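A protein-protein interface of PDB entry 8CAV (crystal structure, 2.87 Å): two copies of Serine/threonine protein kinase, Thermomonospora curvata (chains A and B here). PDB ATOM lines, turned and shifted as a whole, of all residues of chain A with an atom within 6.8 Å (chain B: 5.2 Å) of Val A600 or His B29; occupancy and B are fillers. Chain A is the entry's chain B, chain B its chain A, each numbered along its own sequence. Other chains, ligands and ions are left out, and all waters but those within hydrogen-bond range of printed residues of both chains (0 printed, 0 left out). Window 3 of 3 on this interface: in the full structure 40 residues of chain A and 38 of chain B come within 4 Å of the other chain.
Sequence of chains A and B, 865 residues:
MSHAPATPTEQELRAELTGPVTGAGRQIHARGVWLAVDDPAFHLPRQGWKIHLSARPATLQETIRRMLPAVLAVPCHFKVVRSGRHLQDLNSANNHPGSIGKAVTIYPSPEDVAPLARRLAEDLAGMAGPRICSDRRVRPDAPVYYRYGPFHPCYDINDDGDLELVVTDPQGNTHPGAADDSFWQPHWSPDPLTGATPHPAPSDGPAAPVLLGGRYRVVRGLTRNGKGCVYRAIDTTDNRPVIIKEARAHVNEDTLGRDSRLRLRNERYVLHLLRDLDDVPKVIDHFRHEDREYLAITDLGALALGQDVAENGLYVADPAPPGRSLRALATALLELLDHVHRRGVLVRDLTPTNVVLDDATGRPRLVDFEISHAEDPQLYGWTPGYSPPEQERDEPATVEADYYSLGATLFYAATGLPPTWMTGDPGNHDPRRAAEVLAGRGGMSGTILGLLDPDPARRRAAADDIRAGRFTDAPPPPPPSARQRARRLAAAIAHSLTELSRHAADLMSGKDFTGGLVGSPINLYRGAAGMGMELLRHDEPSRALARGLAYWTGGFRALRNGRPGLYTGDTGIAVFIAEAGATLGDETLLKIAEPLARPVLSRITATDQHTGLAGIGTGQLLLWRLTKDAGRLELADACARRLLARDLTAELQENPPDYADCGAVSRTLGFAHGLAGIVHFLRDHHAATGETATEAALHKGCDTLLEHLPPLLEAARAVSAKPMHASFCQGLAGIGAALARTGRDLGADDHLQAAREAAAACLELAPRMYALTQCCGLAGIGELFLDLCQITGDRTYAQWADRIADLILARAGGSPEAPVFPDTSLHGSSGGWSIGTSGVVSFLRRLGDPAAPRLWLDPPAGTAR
The guanidinium group (NH1) of Arg A603 lies within salt-bridge range of the side-chain carboxylate (OD1) of Asp B38, 3.3 Å away.
The guanidinium group of Arg B31 lies close to the backbone NH of Val A600, at 3.5 Å.
Of the printed residues of chain B, Pro A599 touches Arg B31.
Val A600 touches just these residues of chain B: His B29 and Arg B31.
Of the printed residues of chain B, Ser A602 touches Gln B27 (3.0 Å) and Asp B38 (3.5 Å).
Of the printed residues of chain B, Arg A603 touches Asp B38.
Ile A604 touches none of the printed residues of chain B.
Of the printed residues of chain A, Arg B31 touches Arg A598 (3.7 Å), Pro A599 (3.9 Å) and Val A600 (3.0 Å).
Printed residues of chain A within 4 Å of Asp B38: Ser A602 and Arg A603.
The nearest residue of chain A that does not touch His B29 is Arg A603 (4.2 Å).
Printed residues of chain B that touch a printed residue of chain A: Gln B27, His B29, Arg B31 and Asp B38.
Hydrophobic or aromatic side chains of chain B within 4 Å of the printed part of chain A: His B29.
Of the 11 printed residues of chain A, 5 touch a printed residue of chain B.
Among the printed residues, 7 pairs touch across the chains.
No position is printed for both chains.
Of the 7 pairs that touch across the chains among the printed residues, none has its exchanged pair printed and touching as well.
The backbone carbonyl oxygen (O) of His B29 is in hydrogen-bond range of the backbone NH (N) of Ala B36.
The side-chain carboxylate (OD1) of Asp B38 is in hydrogen-bond range of a ring nitrogen (NE2) of His B29.
Arg B31 touches Arg A598 (NH2 to O, 3.7 Å).
Arg B31 touches Pro A599 (NH2 to C, 3.9 Å).
Val A600 touches His B29.
Gln B27 touches Ser A602.
OD2 of Asp B38 touches CB of Ser A602, 3.5 Å away.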
ATOM      1  N   PRO A 564     -11.828 -15.358 -18.462  1.00  0.00           N
ATOM      2  CA  PRO A 564     -12.863 -15.594 -17.443  1.00  0.00           C
ATOM      3  C   PRO A 564     -12.759 -14.703 -16.218  1.00  0.00           C
ATOM      4  O   PRO A 564     -13.706 -14.677 -15.421  1.00  0.00           O
ATOM      5  CB  PRO A 564     -12.638 -17.063 -17.063  1.00  0.00           C
ATOM      6  CG  PRO A 564     -11.168 -17.252 -17.239  1.00  0.00           C
ATOM      7  CD  PRO A 564     -10.751 -16.366 -18.397  1.00  0.00           C
ATOM      8  N   ARG A 598     -19.497 -18.203 -17.837  1.00  0.00           N
ATOM      9  CA  ARG A 598     -19.721 -19.639 -17.652  1.00  0.00           C
ATOM     10  C   ARG A 598     -18.562 -20.401 -18.283  1.00  0.00           C
ATOM     11  O   ARG A 598     -18.729 -21.135 -19.265  1.00  0.00           O
ATOM     12  CB  ARG A 598     -21.072 -20.049 -18.240  1.00  0.00           C
ATOM     13  CG  ARG A 598     -22.190 -19.866 -17.231  1.00  0.00           C
ATOM     14  CD  ARG A 598     -23.545 -19.581 -17.846  1.00  0.00           C
ATOM     15  NE  ARG A 598     -24.588 -19.757 -16.842  1.00  0.00           N
ATOM     16  CZ  ARG A 598     -25.333 -18.784 -16.336  1.00  0.00           C
ATOM     17  NH1 ARG A 598     -25.252 -17.545 -16.784  1.00  0.00           N
ATOM     18  NH2 ARG A 598     -26.183 -19.061 -15.353  1.00  0.00           N
ATOM     19  N   PRO A 599     -17.364 -20.256 -17.723  1.00  0.00           N
ATOM     20  CA  PRO A 599     -16.171 -20.888 -18.299  1.00  0.00           C
ATOM     21  C   PRO A 599     -16.089 -22.367 -17.948  1.00  0.00           C
ATOM     22  O   PRO A 599     -16.811 -22.862 -17.083  1.00  0.00           O
ATOM     23  CB  PRO A 599     -15.029 -20.108 -17.634  1.00  0.00           C
ATOM     24  CG  PRO A 599     -15.587 -19.792 -16.264  1.00  0.00           C
ATOM     25  CD  PRO A 599     -17.046 -19.473 -16.511  1.00  0.00           C
ATOM     26  N   VAL A 600     -15.178 -23.078 -18.621  1.00  0.00           N
ATOM     27  CA  VAL A 600     -14.794 -24.391 -18.121  1.00  0.00           C
ATOM     28  C   VAL A 600     -13.754 -24.193 -17.033  1.00  0.00           C
ATOM     29  O   VAL A 600     -12.728 -23.539 -17.254  1.00  0.00           O
ATOM     30  CB  VAL A 600     -14.224 -25.317 -19.207  1.00  0.00           C
ATOM     31  CG1 VAL A 600     -14.674 -26.749 -18.888  1.00  0.00           C
ATOM     32  CG2 VAL A 600     -14.587 -24.924 -20.614  1.00  0.00           C
ATOM     33  N   LEU A 601     -14.003 -24.769 -15.876  1.00  0.00           N
ATOM     34  CA  LEU A 601     -13.040 -24.790 -14.788  1.00  0.00           C
ATOM     35  C   LEU A 601     -12.086 -25.965 -14.922  1.00  0.00           C
ATOM     36  O   LEU A 601     -11.086 -26.024 -14.193  1.00  0.00           O
ATOM     37  CB  LEU A 601     -13.814 -24.800 -13.465  1.00  0.00           C
ATOM     38  CG  LEU A 601     -14.901 -23.708 -13.525  1.00  0.00           C
ATOM     39  CD1 LEU A 601     -15.976 -23.855 -12.466  1.00  0.00           C
ATOM     40  CD2 LEU A 601     -14.268 -22.313 -13.440  1.00  0.00           C
ATOM     41  N   SER A 602     -12.369 -26.875 -15.867  1.00  0.00           N
ATOM     42  CA  SER A 602     -11.425 -27.927 -16.229  1.00  0.00           C
ATOM     43  C   SER A 602     -10.159 -27.360 -16.852  1.00  0.00           C
ATOM     44  O   SER A 602      -9.114 -28.020 -16.843  1.00  0.00           O
ATOM     45  CB  SER A 602     -12.079 -28.894 -17.222  1.00  0.00           C
ATOM     46  OG  SER A 602     -13.302 -29.389 -16.714  1.00  0.00           O
ATOM     47  N   ARG A 603     -10.239 -26.167 -17.440  1.00  0.00           N
ATOM     48  CA  ARG A 603      -9.061 -25.419 -17.882  1.00  0.00           C
ATOM     49  C   ARG A 603      -8.723 -24.512 -16.693  1.00  0.00           C
ATOM     50  O   ARG A 603      -8.741 -24.991 -15.555  1.00  0.00           O
ATOM     51  CB  ARG A 603      -9.350 -24.711 -19.206  1.00  0.00           C
ATOM     52  CG  ARG A 603     -10.411 -25.451 -20.085  1.00  0.00           C
ATOM     53  CD  ARG A 603     -10.164 -25.378 -21.610  1.00  0.00           C
ATOM     54  NE  ARG A 603     -11.394 -25.316 -22.403  1.00  0.00           N
ATOM     55  CZ  ARG A 603     -11.867 -26.288 -23.181  1.00  0.00           C
ATOM     56  NH1 ARG A 603     -11.266 -27.463 -23.266  1.00  0.00           N
ATOM     57  NH2 ARG A 603     -12.967 -26.069 -23.896  1.00  0.00           N
ATOM     58  N   ILE A 604      -8.432 -23.229 -16.901  1.00  0.00           N
ATOM     59  CA  ILE A 604      -8.221 -22.303 -15.786  1.00  0.00           C
ATOM     60  C   ILE A 604      -7.226 -22.869 -14.776  1.00  0.00           C
ATOM     61  O   ILE A 604      -7.625 -23.475 -13.774  1.00  0.00           O
ATOM     62  CB  ILE A 604      -9.550 -21.980 -15.060  1.00  0.00           C
ATOM     63  CG1 ILE A 604     -10.583 -21.417 -16.038  1.00  0.00           C
ATOM     64  CG2 ILE A 604      -9.315 -21.010 -13.891  1.00  0.00           C
ATOM     65  CD1 ILE A 604     -11.575 -20.448 -15.415  1.00  0.00           C
ATOM     66  N   LEU A 613      -9.608 -18.971 -10.045  1.00  0.00           N
ATOM     67  CA  LEU A 613     -10.735 -19.661  -9.431  1.00  0.00           C
ATOM     68  C   LEU A 613     -11.319 -18.889  -8.256  1.00  0.00           C
ATOM     69  O   LEU A 613     -12.541 -18.849  -8.082  1.00  0.00           O
ATOM     70  CB  LEU A 613     -10.291 -21.053  -8.982  1.00  0.00           C
ATOM     71  CG  LEU A 613      -9.909 -22.002 -10.119  1.00  0.00           C
ATOM     72  CD1 LEU A 613      -9.156 -23.210  -9.591  1.00  0.00           C
ATOM     73  CD2 LEU A 613     -11.156 -22.432 -10.880  1.00  0.00           C
ATOM     74  N   ILE A 616     -13.219 -15.844  -9.725  1.00  0.00           N
ATOM     75  CA  ILE A 616     -14.372 -16.411 -10.413  1.00  0.00           C
ATOM     76  C   ILE A 616     -15.425 -16.811  -9.390  1.00  0.00           C
ATOM     77  O   ILE A 616     -16.612 -16.514  -9.554  1.00  0.00           O
ATOM     78  CB  ILE A 616     -13.939 -17.592 -11.303  1.00  0.00           C
ATOM     79  CG1 ILE A 616     -12.956 -17.097 -12.376  1.00  0.00           C
ATOM     80  CG2 ILE A 616     -15.143 -18.269 -11.954  1.00  0.00           C
ATOM     81  CD1 ILE A 616     -12.552 -18.140 -13.389  1.00  0.00           C
ATOM     82  N   LEU A 635     -21.214 -22.942  -9.920  1.00  0.00           N
ATOM     83  CA  LEU A 635     -19.889 -22.524 -10.366  1.00  0.00           C
ATOM     84  C   LEU A 635     -19.023 -22.099  -9.186  1.00  0.00           C
ATOM     85  O   LEU A 635     -17.823 -22.397  -9.152  1.00  0.00           O
ATOM     86  CB  LEU A 635     -20.021 -21.398 -11.391  1.00  0.00           C
ATOM     87  CG  LEU A 635     -20.476 -21.875 -12.773  1.00  0.00           C
ATOM     88  CD1 LEU A 635     -21.216 -20.778 -13.519  1.00  0.00           C
ATOM     89  CD2 LEU A 635     -19.276 -22.358 -13.580  1.00  0.00           C
ATOM     90  N   ARG B  14     -22.151 -40.526 -21.002  1.00  0.00           N
ATOM     91  CA  ARG B  14     -21.338 -39.983 -19.923  1.00  0.00           C
ATOM     92  C   ARG B  14     -20.617 -41.085 -19.161  1.00  0.00           C
ATOM     93  O   ARG B  14     -19.454 -40.925 -18.793  1.00  0.00           O
ATOM     94  CB  ARG B  14     -22.210 -39.173 -18.960  1.00  0.00           C
ATOM     95  CG  ARG B  14     -22.593 -37.782 -19.446  1.00  0.00           C
ATOM     96  CD  ARG B  14     -21.891 -36.686 -18.649  1.00  0.00           C
ATOM     97  NE  ARG B  14     -22.639 -35.433 -18.661  1.00  0.00           N
ATOM     98  CZ  ARG B  14     -22.217 -34.300 -18.115  1.00  0.00           C
ATOM     99  NH1 ARG B  14     -21.038 -34.215 -17.521  1.00  0.00           N
ATOM    100  NH2 ARG B  14     -22.997 -33.223 -18.168  1.00  0.00           N
ATOM    101  N   GLN B  27     -10.556 -33.900 -18.107  1.00  0.00           N
ATOM    102  CA  GLN B  27     -11.859 -33.606 -17.516  1.00  0.00           C
ATOM    103  C   GLN B  27     -12.872 -33.211 -18.586  1.00  0.00           C
ATOM    104  O   GLN B  27     -12.535 -32.597 -19.601  1.00  0.00           O
ATOM    105  CB  GLN B  27     -11.728 -32.495 -16.470  1.00  0.00           C
ATOM    106  CG  GLN B  27     -13.003 -32.203 -15.677  1.00  0.00           C
ATOM    107  CD  GLN B  27     -13.494 -33.396 -14.869  1.00  0.00           C
ATOM    108  OE1 GLN B  27     -12.911 -34.477 -14.917  1.00  0.00           O
ATOM    109  NE2 GLN B  27     -14.573 -33.198 -14.122  1.00  0.00           N
ATOM    110  N   ILE B  28     -14.137 -33.558 -18.331  1.00  0.00           N
ATOM    111  CA  ILE B  28     -15.183 -33.511 -19.342  1.00  0.00           C
ATOM    112  C   ILE B  28     -16.286 -32.551 -18.921  1.00  0.00           C
ATOM    113  O   ILE B  28     -16.460 -32.237 -17.741  1.00  0.00           O
ATOM    114  CB  ILE B  28     -15.777 -34.910 -19.605  1.00  0.00           C
ATOM    115  CG1 ILE B  28     -16.712 -35.338 -18.465  1.00  0.00           C
ATOM    116  CG2 ILE B  28     -14.669 -35.924 -19.732  1.00  0.00           C
ATOM    117  CD1 ILE B  28     -18.160 -34.891 -18.627  1.00  0.00           C
ATOM    118  N   HIS B  29     -17.052 -32.108 -19.916  1.00  0.00           N
ATOM    119  CA  HIS B  29     -18.205 -31.244 -19.665  1.00  0.00           C
ATOM    120  C   HIS B  29     -19.005 -31.115 -20.950  1.00  0.00           C
ATOM    121  O   HIS B  29     -18.478 -31.334 -22.040  1.00  0.00           O
ATOM    122  CB  HIS B  29     -17.767 -29.864 -19.197  1.00  0.00           C
ATOM    123  CG  HIS B  29     -16.812 -29.217 -20.143  1.00  0.00           C
ATOM    124  ND1 HIS B  29     -17.181 -28.214 -21.012  1.00  0.00           N
ATOM    125  CD2 HIS B  29     -15.512 -29.487 -20.406  1.00  0.00           C
ATOM    126  CE1 HIS B  29     -16.137 -27.868 -21.744  1.00  0.00           C
ATOM    127  NE2 HIS B  29     -15.113 -28.624 -21.396  1.00  0.00           N
ATOM    128  N   ALA B  30     -20.268 -30.713 -20.824  1.00  0.00           N
ATOM    129  CA  ALA B  30     -21.145 -30.596 -21.982  1.00  0.00           C
ATOM    130  C   ALA B  30     -21.692 -29.182 -22.135  1.00  0.00           C
ATOM    131  O   ALA B  30     -22.022 -28.515 -21.149  1.00  0.00           O
ATOM    132  CB  ALA B  30     -22.307 -31.595 -21.894  1.00  0.00           C
ATOM    133  N   ARG B  31     -21.785 -28.749 -23.392  1.00  0.00           N
ATOM    134  CA  ARG B  31     -22.373 -27.469 -23.762  1.00  0.00           C
ATOM    135  C   ARG B  31     -23.221 -27.644 -25.012  1.00  0.00           C
ATOM    136  O   ARG B  31     -22.840 -28.381 -25.922  1.00  0.00           O
ATOM    137  CB  ARG B  31     -21.322 -26.402 -24.071  1.00  0.00           C
ATOM    138  CG  ARG B  31     -20.470 -25.934 -22.922  1.00  0.00           C
ATOM    139  CD  ARG B  31     -19.537 -24.847 -23.432  1.00  0.00           C
ATOM    140  NE  ARG B  31     -18.589 -24.386 -22.428  1.00  0.00           N
ATOM    141  CZ  ARG B  31     -17.619 -23.514 -22.665  1.00  0.00           C
ATOM    142  NH1 ARG B  31     -17.440 -22.987 -23.866  1.00  0.00           N
ATOM    143  NH2 ARG B  31     -16.806 -23.161 -21.674  1.00  0.00           N
ATOM    144  N   TRP B  34     -22.941 -30.975 -27.050  1.00  0.00           N
ATOM    145  CA  TRP B  34     -21.698 -31.729 -27.047  1.00  0.00           C
ATOM    146  C   TRP B  34     -21.243 -32.050 -25.631  1.00  0.00           C
ATOM    147  O   TRP B  34     -21.563 -31.342 -24.676  1.00  0.00           O
ATOM    148  CB  TRP B  34     -20.579 -30.961 -27.770  1.00  0.00           C
ATOM    149  CG  TRP B  34     -20.925 -30.576 -29.173  1.00  0.00           C
ATOM    150  CD1 TRP B  34     -21.494 -29.406 -29.583  1.00  0.00           C
ATOM    151  CD2 TRP B  34     -20.723 -31.360 -30.356  1.00  0.00           C
ATOM    152  NE1 TRP B  34     -21.662 -29.412 -30.946  1.00  0.00           N
ATOM    153  CE2 TRP B  34     -21.196 -30.600 -31.446  1.00  0.00           C
ATOM    154  CE3 TRP B  34     -20.189 -32.628 -30.601  1.00  0.00           C
ATOM    155  CZ2 TRP B  34     -21.151 -31.067 -32.758  1.00  0.00           C
ATOM    156  CZ3 TRP B  34     -20.146 -33.091 -31.905  1.00  0.00           C
ATOM    157  CH2 TRP B  34     -20.623 -32.311 -32.966  1.00  0.00           C
ATOM    158  N   LEU B  35     -20.489 -33.147 -25.534  1.00  0.00           N
ATOM    159  CA  LEU B  35     -19.819 -33.642 -24.339  1.00  0.00           C
ATOM    160  C   LEU B  35     -18.347 -33.760 -24.716  1.00  0.00           C
ATOM    161  O   LEU B  35     -17.975 -34.637 -25.502  1.00  0.00           O
ATOM    162  CB  LEU B  35     -20.386 -34.994 -23.911  1.00  0.00           C
ATOM    163  CG  LEU B  35     -21.616 -35.038 -23.004  1.00  0.00           C
ATOM    164  CD1 LEU B  35     -22.443 -36.296 -23.224  1.00  0.00           C
ATOM    165  CD2 LEU B  35     -21.163 -34.969 -21.552  1.00  0.00           C
ATOM    166  N   ALA B  36     -17.513 -32.861 -24.201  1.00  0.00           N
ATOM    167  CA  ALA B  36     -16.150 -32.709 -24.679  1.00  0.00           C
ATOM    168  C   ALA B  36     -15.144 -32.989 -23.572  1.00  0.00           C
ATOM    169  O   ALA B  36     -15.387 -32.709 -22.387  1.00  0.00           O
ATOM    170  CB  ALA B  36     -15.916 -31.299 -25.239  1.00  0.00           C
ATOM    171  N   ASP B  38     -10.857 -32.584 -22.749  1.00  0.00           N
ATOM    172  CA  ASP B  38      -9.757 -31.675 -23.048  1.00  0.00           C
ATOM    173  C   ASP B  38      -8.480 -32.175 -22.385  1.00  0.00           C
ATOM    174  O   ASP B  38      -8.418 -32.294 -21.157  1.00  0.00           O
ATOM    175  CB  ASP B  38     -10.079 -30.256 -22.563  1.00  0.00           C
ATOM    176  CG  ASP B  38     -11.249 -30.221 -21.593  1.00  0.00           C
ATOM    177  OD1 ASP B  38     -12.405 -30.364 -22.048  1.00  0.00           O
ATOM    178  OD2 ASP B  38     -11.014 -30.071 -20.375  1.00  0.00           O
